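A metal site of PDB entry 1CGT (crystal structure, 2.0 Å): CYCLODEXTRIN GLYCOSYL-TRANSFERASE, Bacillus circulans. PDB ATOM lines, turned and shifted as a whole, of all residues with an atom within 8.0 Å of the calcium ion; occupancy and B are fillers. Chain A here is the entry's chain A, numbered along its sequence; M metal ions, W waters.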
ATOM      1  N   PRO A 138       4.204   9.078  16.363  1.00  0.00           N
ATOM      2  CA  PRO A 138       5.224   8.335  15.648  1.00  0.00           C
ATOM      3  C   PRO A 138       6.639   8.739  16.004  1.00  0.00           C
ATOM      4  O   PRO A 138       7.587   8.203  15.402  1.00  0.00           O
ATOM      5  CB  PRO A 138       4.982   8.560  14.169  1.00  0.00           C
ATOM      6  CG  PRO A 138       3.954   9.652  14.099  1.00  0.00           C
ATOM      7  CD  PRO A 138       3.715  10.163  15.519  1.00  0.00           C
ATOM      8  N   ASN A 139       6.856   9.698  16.918  1.00  0.00           N
ATOM      9  CA  ASN A 139       8.197  10.126  17.197  1.00  0.00           C
ATOM     10  C   ASN A 139       8.969   9.117  18.042  1.00  0.00           C
ATOM     11  O   ASN A 139      10.205   9.022  17.881  1.00  0.00           O
ATOM     12  CB  ASN A 139       8.208  11.524  17.930  1.00  0.00           C
ATOM     13  CG  ASN A 139       9.617  12.010  18.297  1.00  0.00           C
ATOM     14  OD1 ASN A 139      10.492  12.323  17.479  1.00  0.00           O
ATOM     15  ND2 ASN A 139       9.963  12.078  19.582  1.00  0.00           N
ATOM     16  N   HIS A 140       8.298   8.314  18.867  1.00  0.00           N
ATOM     17  CA  HIS A 140       9.026   7.549  19.902  1.00  0.00           C
ATOM     18  C   HIS A 140       8.175   6.392  20.377  1.00  0.00           C
ATOM     19  O   HIS A 140       6.950   6.381  20.087  1.00  0.00           O
ATOM     20  CB  HIS A 140       9.357   8.434  21.148  1.00  0.00           C
ATOM     21  CG  HIS A 140       8.127   9.144  21.739  1.00  0.00           C
ATOM     22  ND1 HIS A 140       7.744  10.410  21.612  1.00  0.00           N
ATOM     23  CD2 HIS A 140       7.131   8.502  22.439  1.00  0.00           C
ATOM     24  CE1 HIS A 140       6.568  10.564  22.167  1.00  0.00           C
ATOM     25  NE2 HIS A 140       6.220   9.416  22.665  1.00  0.00           N
ATOM     26  N   HIS A 176      17.346   6.274  17.299  1.00  0.00           N
ATOM     27  CA  HIS A 176      18.510   7.126  17.278  1.00  0.00           C
ATOM     28  C   HIS A 176      19.289   6.848  18.550  1.00  0.00           C
ATOM     29  O   HIS A 176      18.718   6.556  19.592  1.00  0.00           O
ATOM     30  CB  HIS A 176      18.150   8.600  17.289  1.00  0.00           C
ATOM     31  CG  HIS A 176      17.581   9.093  15.961  1.00  0.00           C
ATOM     32  ND1 HIS A 176      16.477   9.796  15.774  1.00  0.00           N
ATOM     33  CD2 HIS A 176      18.151   8.937  14.717  1.00  0.00           C
ATOM     34  CE1 HIS A 176      16.338  10.080  14.500  1.00  0.00           C
ATOM     35  NE2 HIS A 176      17.352   9.545  13.857  1.00  0.00           N
ATOM     36  N   GLU A 187      17.477  21.100  14.732  1.00  0.00           N
ATOM     37  CA  GLU A 187      18.160  19.871  14.391  1.00  0.00           C
ATOM     38  C   GLU A 187      18.368  18.980  15.628  1.00  0.00           C
ATOM     39  O   GLU A 187      18.100  17.766  15.634  1.00  0.00           O
ATOM     40  CB  GLU A 187      19.500  20.238  13.779  1.00  0.00           C
ATOM     41  CG  GLU A 187      20.254  18.982  13.371  1.00  0.00           C
ATOM     42  CD  GLU A 187      21.637  19.186  12.782  1.00  0.00           C
ATOM     43  OE1 GLU A 187      22.057  20.304  12.501  1.00  0.00           O
ATOM     44  OE2 GLU A 187      22.298  18.188  12.571  1.00  0.00           O
ATOM     45  N   ASN A 188      18.898  19.586  16.682  1.00  0.00           N
ATOM     46  CA  ASN A 188      19.183  18.895  17.925  1.00  0.00           C
ATOM     47  C   ASN A 188      17.910  18.267  18.463  1.00  0.00           C
ATOM     48  O   ASN A 188      17.911  17.117  18.912  1.00  0.00           O
ATOM     49  CB  ASN A 188      19.753  19.899  18.913  1.00  0.00           C
ATOM     50  CG  ASN A 188      20.236  19.217  20.191  1.00  0.00           C
ATOM     51  OD1 ASN A 188      21.434  19.055  20.469  1.00  0.00           O
ATOM     52  ND2 ASN A 188      19.348  18.800  21.063  1.00  0.00           N
ATOM     53  N   GLY A 189      16.767  18.961  18.416  1.00  0.00           N
ATOM     54  CA  GLY A 189      15.516  18.396  18.889  1.00  0.00           C
ATOM     55  C   GLY A 189      14.912  17.346  17.973  1.00  0.00           C
ATOM     56  O   GLY A 189      13.985  16.659  18.427  1.00  0.00           O
ATOM     57  N   ILE A 190      15.351  17.151  16.730  1.00  0.00           N
ATOM     58  CA  ILE A 190      14.796  16.134  15.858  1.00  0.00           C
ATOM     59  C   ILE A 190      15.550  14.818  15.997  1.00  0.00           C
ATOM     60  O   ILE A 190      14.926  13.733  16.005  1.00  0.00           O
ATOM     61  CB  ILE A 190      14.847  16.644  14.363  1.00  0.00           C
ATOM     62  CG1 ILE A 190      13.844  17.793  14.178  1.00  0.00           C
ATOM     63  CG2 ILE A 190      14.521  15.516  13.393  1.00  0.00           C
ATOM     64  CD1 ILE A 190      13.973  18.592  12.872  1.00  0.00           C
ATOM     65  N   TYR A 191      16.862  14.848  16.072  1.00  0.00           N
ATOM     66  CA  TYR A 191      17.608  13.592  15.972  1.00  0.00           C
ATOM     67  C   TYR A 191      18.172  13.037  17.274  1.00  0.00           C
ATOM     68  O   TYR A 191      18.928  12.065  17.281  1.00  0.00           O
ATOM     69  CB  TYR A 191      18.747  13.758  14.903  1.00  0.00           C
ATOM     70  CG  TYR A 191      18.179  14.014  13.508  1.00  0.00           C
ATOM     71  CD1 TYR A 191      17.608  12.991  12.770  1.00  0.00           C
ATOM     72  CD2 TYR A 191      18.225  15.305  13.000  1.00  0.00           C
ATOM     73  CE1 TYR A 191      17.067  13.233  11.518  1.00  0.00           C
ATOM     74  CE2 TYR A 191      17.700  15.554  11.744  1.00  0.00           C
ATOM     75  CZ  TYR A 191      17.125  14.521  11.023  1.00  0.00           C
ATOM     76  OH  TYR A 191      16.622  14.792   9.738  1.00  0.00           O
ATOM     77  N   LYS A 192      17.786  13.662  18.377  1.00  0.00           N
ATOM     78  CA  LYS A 192      18.122  13.173  19.704  1.00  0.00           C
ATOM     79  C   LYS A 192      16.824  12.856  20.440  1.00  0.00           C
ATOM     80  O   LYS A 192      15.708  13.214  20.002  1.00  0.00           O
ATOM     81  CB  LYS A 192      18.887  14.218  20.483  1.00  0.00           C
ATOM     82  CG  LYS A 192      20.205  14.557  19.813  1.00  0.00           C
ATOM     83  CD  LYS A 192      21.040  15.328  20.772  1.00  0.00           C
ATOM     84  CE  LYS A 192      22.363  15.376  20.065  1.00  0.00           C
ATOM     85  NZ  LYS A 192      23.422  15.615  21.013  1.00  0.00           N
ATOM     86  N   ASN A 193      16.920  12.145  21.561  1.00  0.00           N
ATOM     87  CA  ASN A 193      15.791  11.764  22.377  1.00  0.00           C
ATOM     88  C   ASN A 193      15.133  12.920  23.109  1.00  0.00           C
ATOM     89  O   ASN A 193      15.785  13.838  23.629  1.00  0.00           O
ATOM     90  CB  ASN A 193      16.179  10.731  23.449  1.00  0.00           C
ATOM     91  CG  ASN A 193      16.676   9.405  22.896  1.00  0.00           C
ATOM     92  OD1 ASN A 193      16.484   9.034  21.737  1.00  0.00           O
ATOM     93  ND2 ASN A 193      17.405   8.637  23.691  1.00  0.00           N
ATOM     94  N   LEU A 194      13.804  12.903  23.144  1.00  0.00           N
ATOM     95  CA  LEU A 194      13.085  13.804  24.020  1.00  0.00           C
ATOM     96  C   LEU A 194      13.119  13.130  25.372  1.00  0.00           C
ATOM     97  O   LEU A 194      12.471  12.105  25.622  1.00  0.00           O
ATOM     98  CB  LEU A 194      11.664  13.928  23.636  1.00  0.00           C
ATOM     99  CG  LEU A 194      11.330  14.494  22.319  1.00  0.00           C
ATOM    100  CD1 LEU A 194       9.816  14.612  22.252  1.00  0.00           C
ATOM    101  CD2 LEU A 194      12.002  15.849  22.160  1.00  0.00           C
ATOM    102  N   LEU A 197      12.728   9.239  26.056  1.00  0.00           N
ATOM    103  CA  LEU A 197      11.906   8.503  25.132  1.00  0.00           C
ATOM    104  C   LEU A 197      12.728   8.020  23.957  1.00  0.00           C
ATOM    105  O   LEU A 197      13.375   8.856  23.299  1.00  0.00           O
ATOM    106  CB  LEU A 197      10.784   9.389  24.667  1.00  0.00           C
ATOM    107  CG  LEU A 197       9.843   9.822  25.770  1.00  0.00           C
ATOM    108  CD1 LEU A 197       8.889  10.854  25.245  1.00  0.00           C
ATOM    109  CD2 LEU A 197       9.054   8.628  26.275  1.00  0.00           C
ATOM    110  N   ALA A 198      12.689   6.726  23.657  1.00  0.00           N
ATOM    111  CA  ALA A 198      13.428   6.114  22.574  1.00  0.00           C
ATOM    112  C   ALA A 198      12.968   6.675  21.208  1.00  0.00           C
ATOM    113  O   ALA A 198      11.836   6.417  20.764  1.00  0.00           O
ATOM    114  CB  ALA A 198      13.196   4.590  22.634  1.00  0.00           C
ATOM    115  N   ASP A 199      13.859   7.445  20.566  1.00  0.00           N
ATOM    116  CA  ASP A 199      13.551   8.155  19.339  1.00  0.00           C
ATOM    117  C   ASP A 199      13.604   7.300  18.084  1.00  0.00           C
ATOM    118  O   ASP A 199      14.679   6.756  17.773  1.00  0.00           O
ATOM    119  CB  ASP A 199      14.526   9.307  19.227  1.00  0.00           C
ATOM    120  CG  ASP A 199      13.917  10.486  18.501  1.00  0.00           C
ATOM    121  OD1 ASP A 199      12.938  11.047  18.967  1.00  0.00           O
ATOM    122  OD2 ASP A 199      14.444  10.857  17.470  1.00  0.00           O
ATOM    123  N   PHE A 200      12.515   7.174  17.336  1.00  0.00           N
ATOM    124  CA  PHE A 200      12.550   6.441  16.088  1.00  0.00           C
ATOM    125  C   PHE A 200      13.445   7.068  15.031  1.00  0.00           C
ATOM    126  O   PHE A 200      13.539   8.304  14.908  1.00  0.00           O
ATOM    127  CB  PHE A 200      11.186   6.331  15.453  1.00  0.00           C
ATOM    128  CG  PHE A 200      10.358   5.245  16.094  1.00  0.00           C
ATOM    129  CD1 PHE A 200      10.759   3.926  15.994  1.00  0.00           C
ATOM    130  CD2 PHE A 200       9.185   5.560  16.756  1.00  0.00           C
ATOM    131  CE1 PHE A 200       9.975   2.924  16.542  1.00  0.00           C
ATOM    132  CE2 PHE A 200       8.429   4.547  17.293  1.00  0.00           C
ATOM    133  CZ  PHE A 200       8.808   3.231  17.189  1.00  0.00           C
ATOM    134  N   ASN A 201      14.111   6.197  14.276  1.00  0.00           N
ATOM    135  CA  ASN A 201      14.918   6.562  13.115  1.00  0.00           C
ATOM    136  C   ASN A 201      14.006   6.255  11.918  1.00  0.00           C
ATOM    137  O   ASN A 201      13.896   5.143  11.407  1.00  0.00           O
ATOM    138  CB  ASN A 201      16.183   5.715  13.083  1.00  0.00           C
ATOM    139  CG  ASN A 201      16.880   5.872  11.747  1.00  0.00           C
ATOM    140  OD1 ASN A 201      16.626   6.808  11.000  1.00  0.00           O
ATOM    141  ND2 ASN A 201      17.754   4.955  11.391  1.00  0.00           N
ATOM    142  N   HIS A 202      13.329   7.279  11.380  1.00  0.00           N
ATOM    143  CA  HIS A 202      12.359   7.067  10.317  1.00  0.00           C
ATOM    144  C   HIS A 202      13.039   6.876   8.965  1.00  0.00           C
ATOM    145  O   HIS A 202      12.369   6.606   7.972  1.00  0.00           O
ATOM    146  CB  HIS A 202      11.383   8.245  10.240  1.00  0.00           C
ATOM    147  CG  HIS A 202      10.578   8.456  11.511  1.00  0.00           C
ATOM    148  ND1 HIS A 202      10.838   9.347  12.456  1.00  0.00           N
ATOM    149  CD2 HIS A 202       9.451   7.746  11.874  1.00  0.00           C
ATOM    150  CE1 HIS A 202       9.913   9.222  13.392  1.00  0.00           C
ATOM    151  NE2 HIS A 202       9.087   8.265  13.040  1.00  0.00           N
ATOM    152  N   ALA A 230       4.324  15.896  18.734  1.00  0.00           N
ATOM    153  CA  ALA A 230       5.747  16.230  18.612  1.00  0.00           C
ATOM    154  C   ALA A 230       6.277  16.434  17.198  1.00  0.00           C
ATOM    155  O   ALA A 230       7.397  15.987  16.849  1.00  0.00           O
ATOM    156  CB  ALA A 230       6.611  15.122  19.318  1.00  0.00           C
ATOM    157  N   VAL A 231       5.501  17.185  16.392  1.00  0.00           N
ATOM    158  CA  VAL A 231       5.863  17.345  14.979  1.00  0.00           C
ATOM    159  C   VAL A 231       7.151  18.153  14.811  1.00  0.00           C
ATOM    160  O   VAL A 231       7.889  18.040  13.828  1.00  0.00           O
ATOM    161  CB  VAL A 231       4.700  18.011  14.126  1.00  0.00           C
ATOM    162  CG1 VAL A 231       3.541  17.007  14.191  1.00  0.00           C
ATOM    163  CG2 VAL A 231       4.351  19.464  14.531  1.00  0.00           C
ATOM    164  N   LYS A 232       7.511  18.931  15.813  1.00  0.00           N
ATOM    165  CA  LYS A 232       8.739  19.687  15.860  1.00  0.00           C
ATOM    166  C   LYS A 232       9.932  18.747  16.051  1.00  0.00           C
ATOM    167  O   LYS A 232      11.080  19.170  15.931  1.00  0.00           O
ATOM    168  CB  LYS A 232       8.623  20.646  17.016  1.00  0.00           C
ATOM    169  CG  LYS A 232       9.723  21.657  17.034  1.00  0.00           C
ATOM    170  CD  LYS A 232       9.544  22.545  18.227  1.00  0.00           C
ATOM    171  CE  LYS A 232      10.852  23.325  18.096  1.00  0.00           C
ATOM    172  NZ  LYS A 232      10.967  24.350  19.127  1.00  0.00           N
ATOM    173  N   HIS A 233       9.712  17.470  16.378  1.00  0.00           N
ATOM    174  CA  HIS A 233      10.789  16.600  16.769  1.00  0.00           C
ATOM    175  C   HIS A 233      10.977  15.523  15.777  1.00  0.00           C
ATOM    176  O   HIS A 233      11.721  14.552  16.055  1.00  0.00           O
ATOM    177  CB  HIS A 233      10.474  16.036  18.197  1.00  0.00           C
ATOM    178  CG  HIS A 233      10.549  17.196  19.165  1.00  0.00           C
ATOM    179  ND1 HIS A 233      11.644  17.907  19.483  1.00  0.00           N
ATOM    180  CD2 HIS A 233       9.488  17.806  19.827  1.00  0.00           C
ATOM    181  CE1 HIS A 233      11.310  18.907  20.295  1.00  0.00           C
ATOM    182  NE2 HIS A 233      10.016  18.828  20.493  1.00  0.00           N
ATOM    183  N   MET A 234      10.314  15.612  14.628  1.00  0.00           N
ATOM    184  CA  MET A 234      10.473  14.651  13.566  1.00  0.00           C
ATOM    185  C   MET A 234      10.809  15.451  12.316  1.00  0.00           C
ATOM    186  O   MET A 234      10.456  16.645  12.238  1.00  0.00           O
ATOM    187  CB  MET A 234       9.190  13.853  13.324  1.00  0.00           C
ATOM    188  CG  MET A 234       8.935  12.879  14.447  1.00  0.00           C
ATOM    189  SD  MET A 234       7.423  11.988  14.138  1.00  0.00           S
ATOM    190  CE  MET A 234       6.250  13.249  14.578  1.00  0.00           C
ATOM    191  N   PRO A 235      11.517  14.891  11.326  1.00  0.00           N
ATOM    192  CA  PRO A 235      11.902  15.615  10.093  1.00  0.00           C
ATOM    193  C   PRO A 235      10.643  16.023   9.289  1.00  0.00           C
ATOM    194  O   PRO A 235       9.769  15.164   9.040  1.00  0.00           O
ATOM    195  CB  PRO A 235      12.814  14.628   9.326  1.00  0.00           C
ATOM    196  CG  PRO A 235      13.206  13.585  10.370  1.00  0.00           C
ATOM    197  CD  PRO A 235      12.019  13.514  11.302  1.00  0.00           C
HETATM  198 CA    CA M   1      12.650  12.526  16.850  1.00  0.00          CA
HETATM  199  O   HOH W   1      13.334  12.369  14.532  1.00  0.00           O
HETATM  200  O   HOH W   2      13.281  13.827  18.574  1.00  0.00           O
HETATM  201  O   HOH W   3      11.874  10.538  16.149  1.00  0.00           O
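SD of Met 234 lies within hydrogen-bond range of N of Asn 139, at 3.6 Å. The backbone NH (N) of Phe 200 lies within hydrogen-bond range of the backbone carbonyl oxygen (O) of Asn 139 (3.0 Å). ND2 of Asn 139 sits at hydrogen-bond distance from ND1 of His 140 (3.4 Å). The backbone carbonyl oxygen of Gly 189 lies within hydrogen-bond range of a ring nitrogen (ND1) of His 233 (2.9 Å). The backbone carbonyl oxygen (O) of Asp 199 lies within hydrogen-bond range of the backbone NH (N) of His 176. The backbone NH (N) of Asp 199 sits close to the side-chain amide oxygen (OD1) of Asn 193, 3.3 Å away.
Four residues have an atom within 4 Å of the calcium ion: Asn 139, Ile 190, Asp 199 and His 233. The nearest printed residue that does not touch the calcium ion is Met 234 (4.4 Å).
The calcium ion is bound by water W3 (2.2 Å), water W2 (2.3 Å), the side-chain amide oxygen (OD1) of Asn 139 (2.3 Å), the backbone carbonyl oxygen (O) of His 233 (2.4 Å), water W1 (2.4 Å), the side-chain carboxylate (OD2) of Asp 199 (2.5 Å), the side-chain carboxylate (OD1) of Asp 199 (2.6 Å) and the backbone carbonyl oxygen (O) of Ile 190 (2.7 Å).
Water W3 bridges the backbone carbonyl oxygen (O) of Asn 139 (2.8 Å) and the backbone carbonyl oxygen (O) of Phe 200 (3.1 Å).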
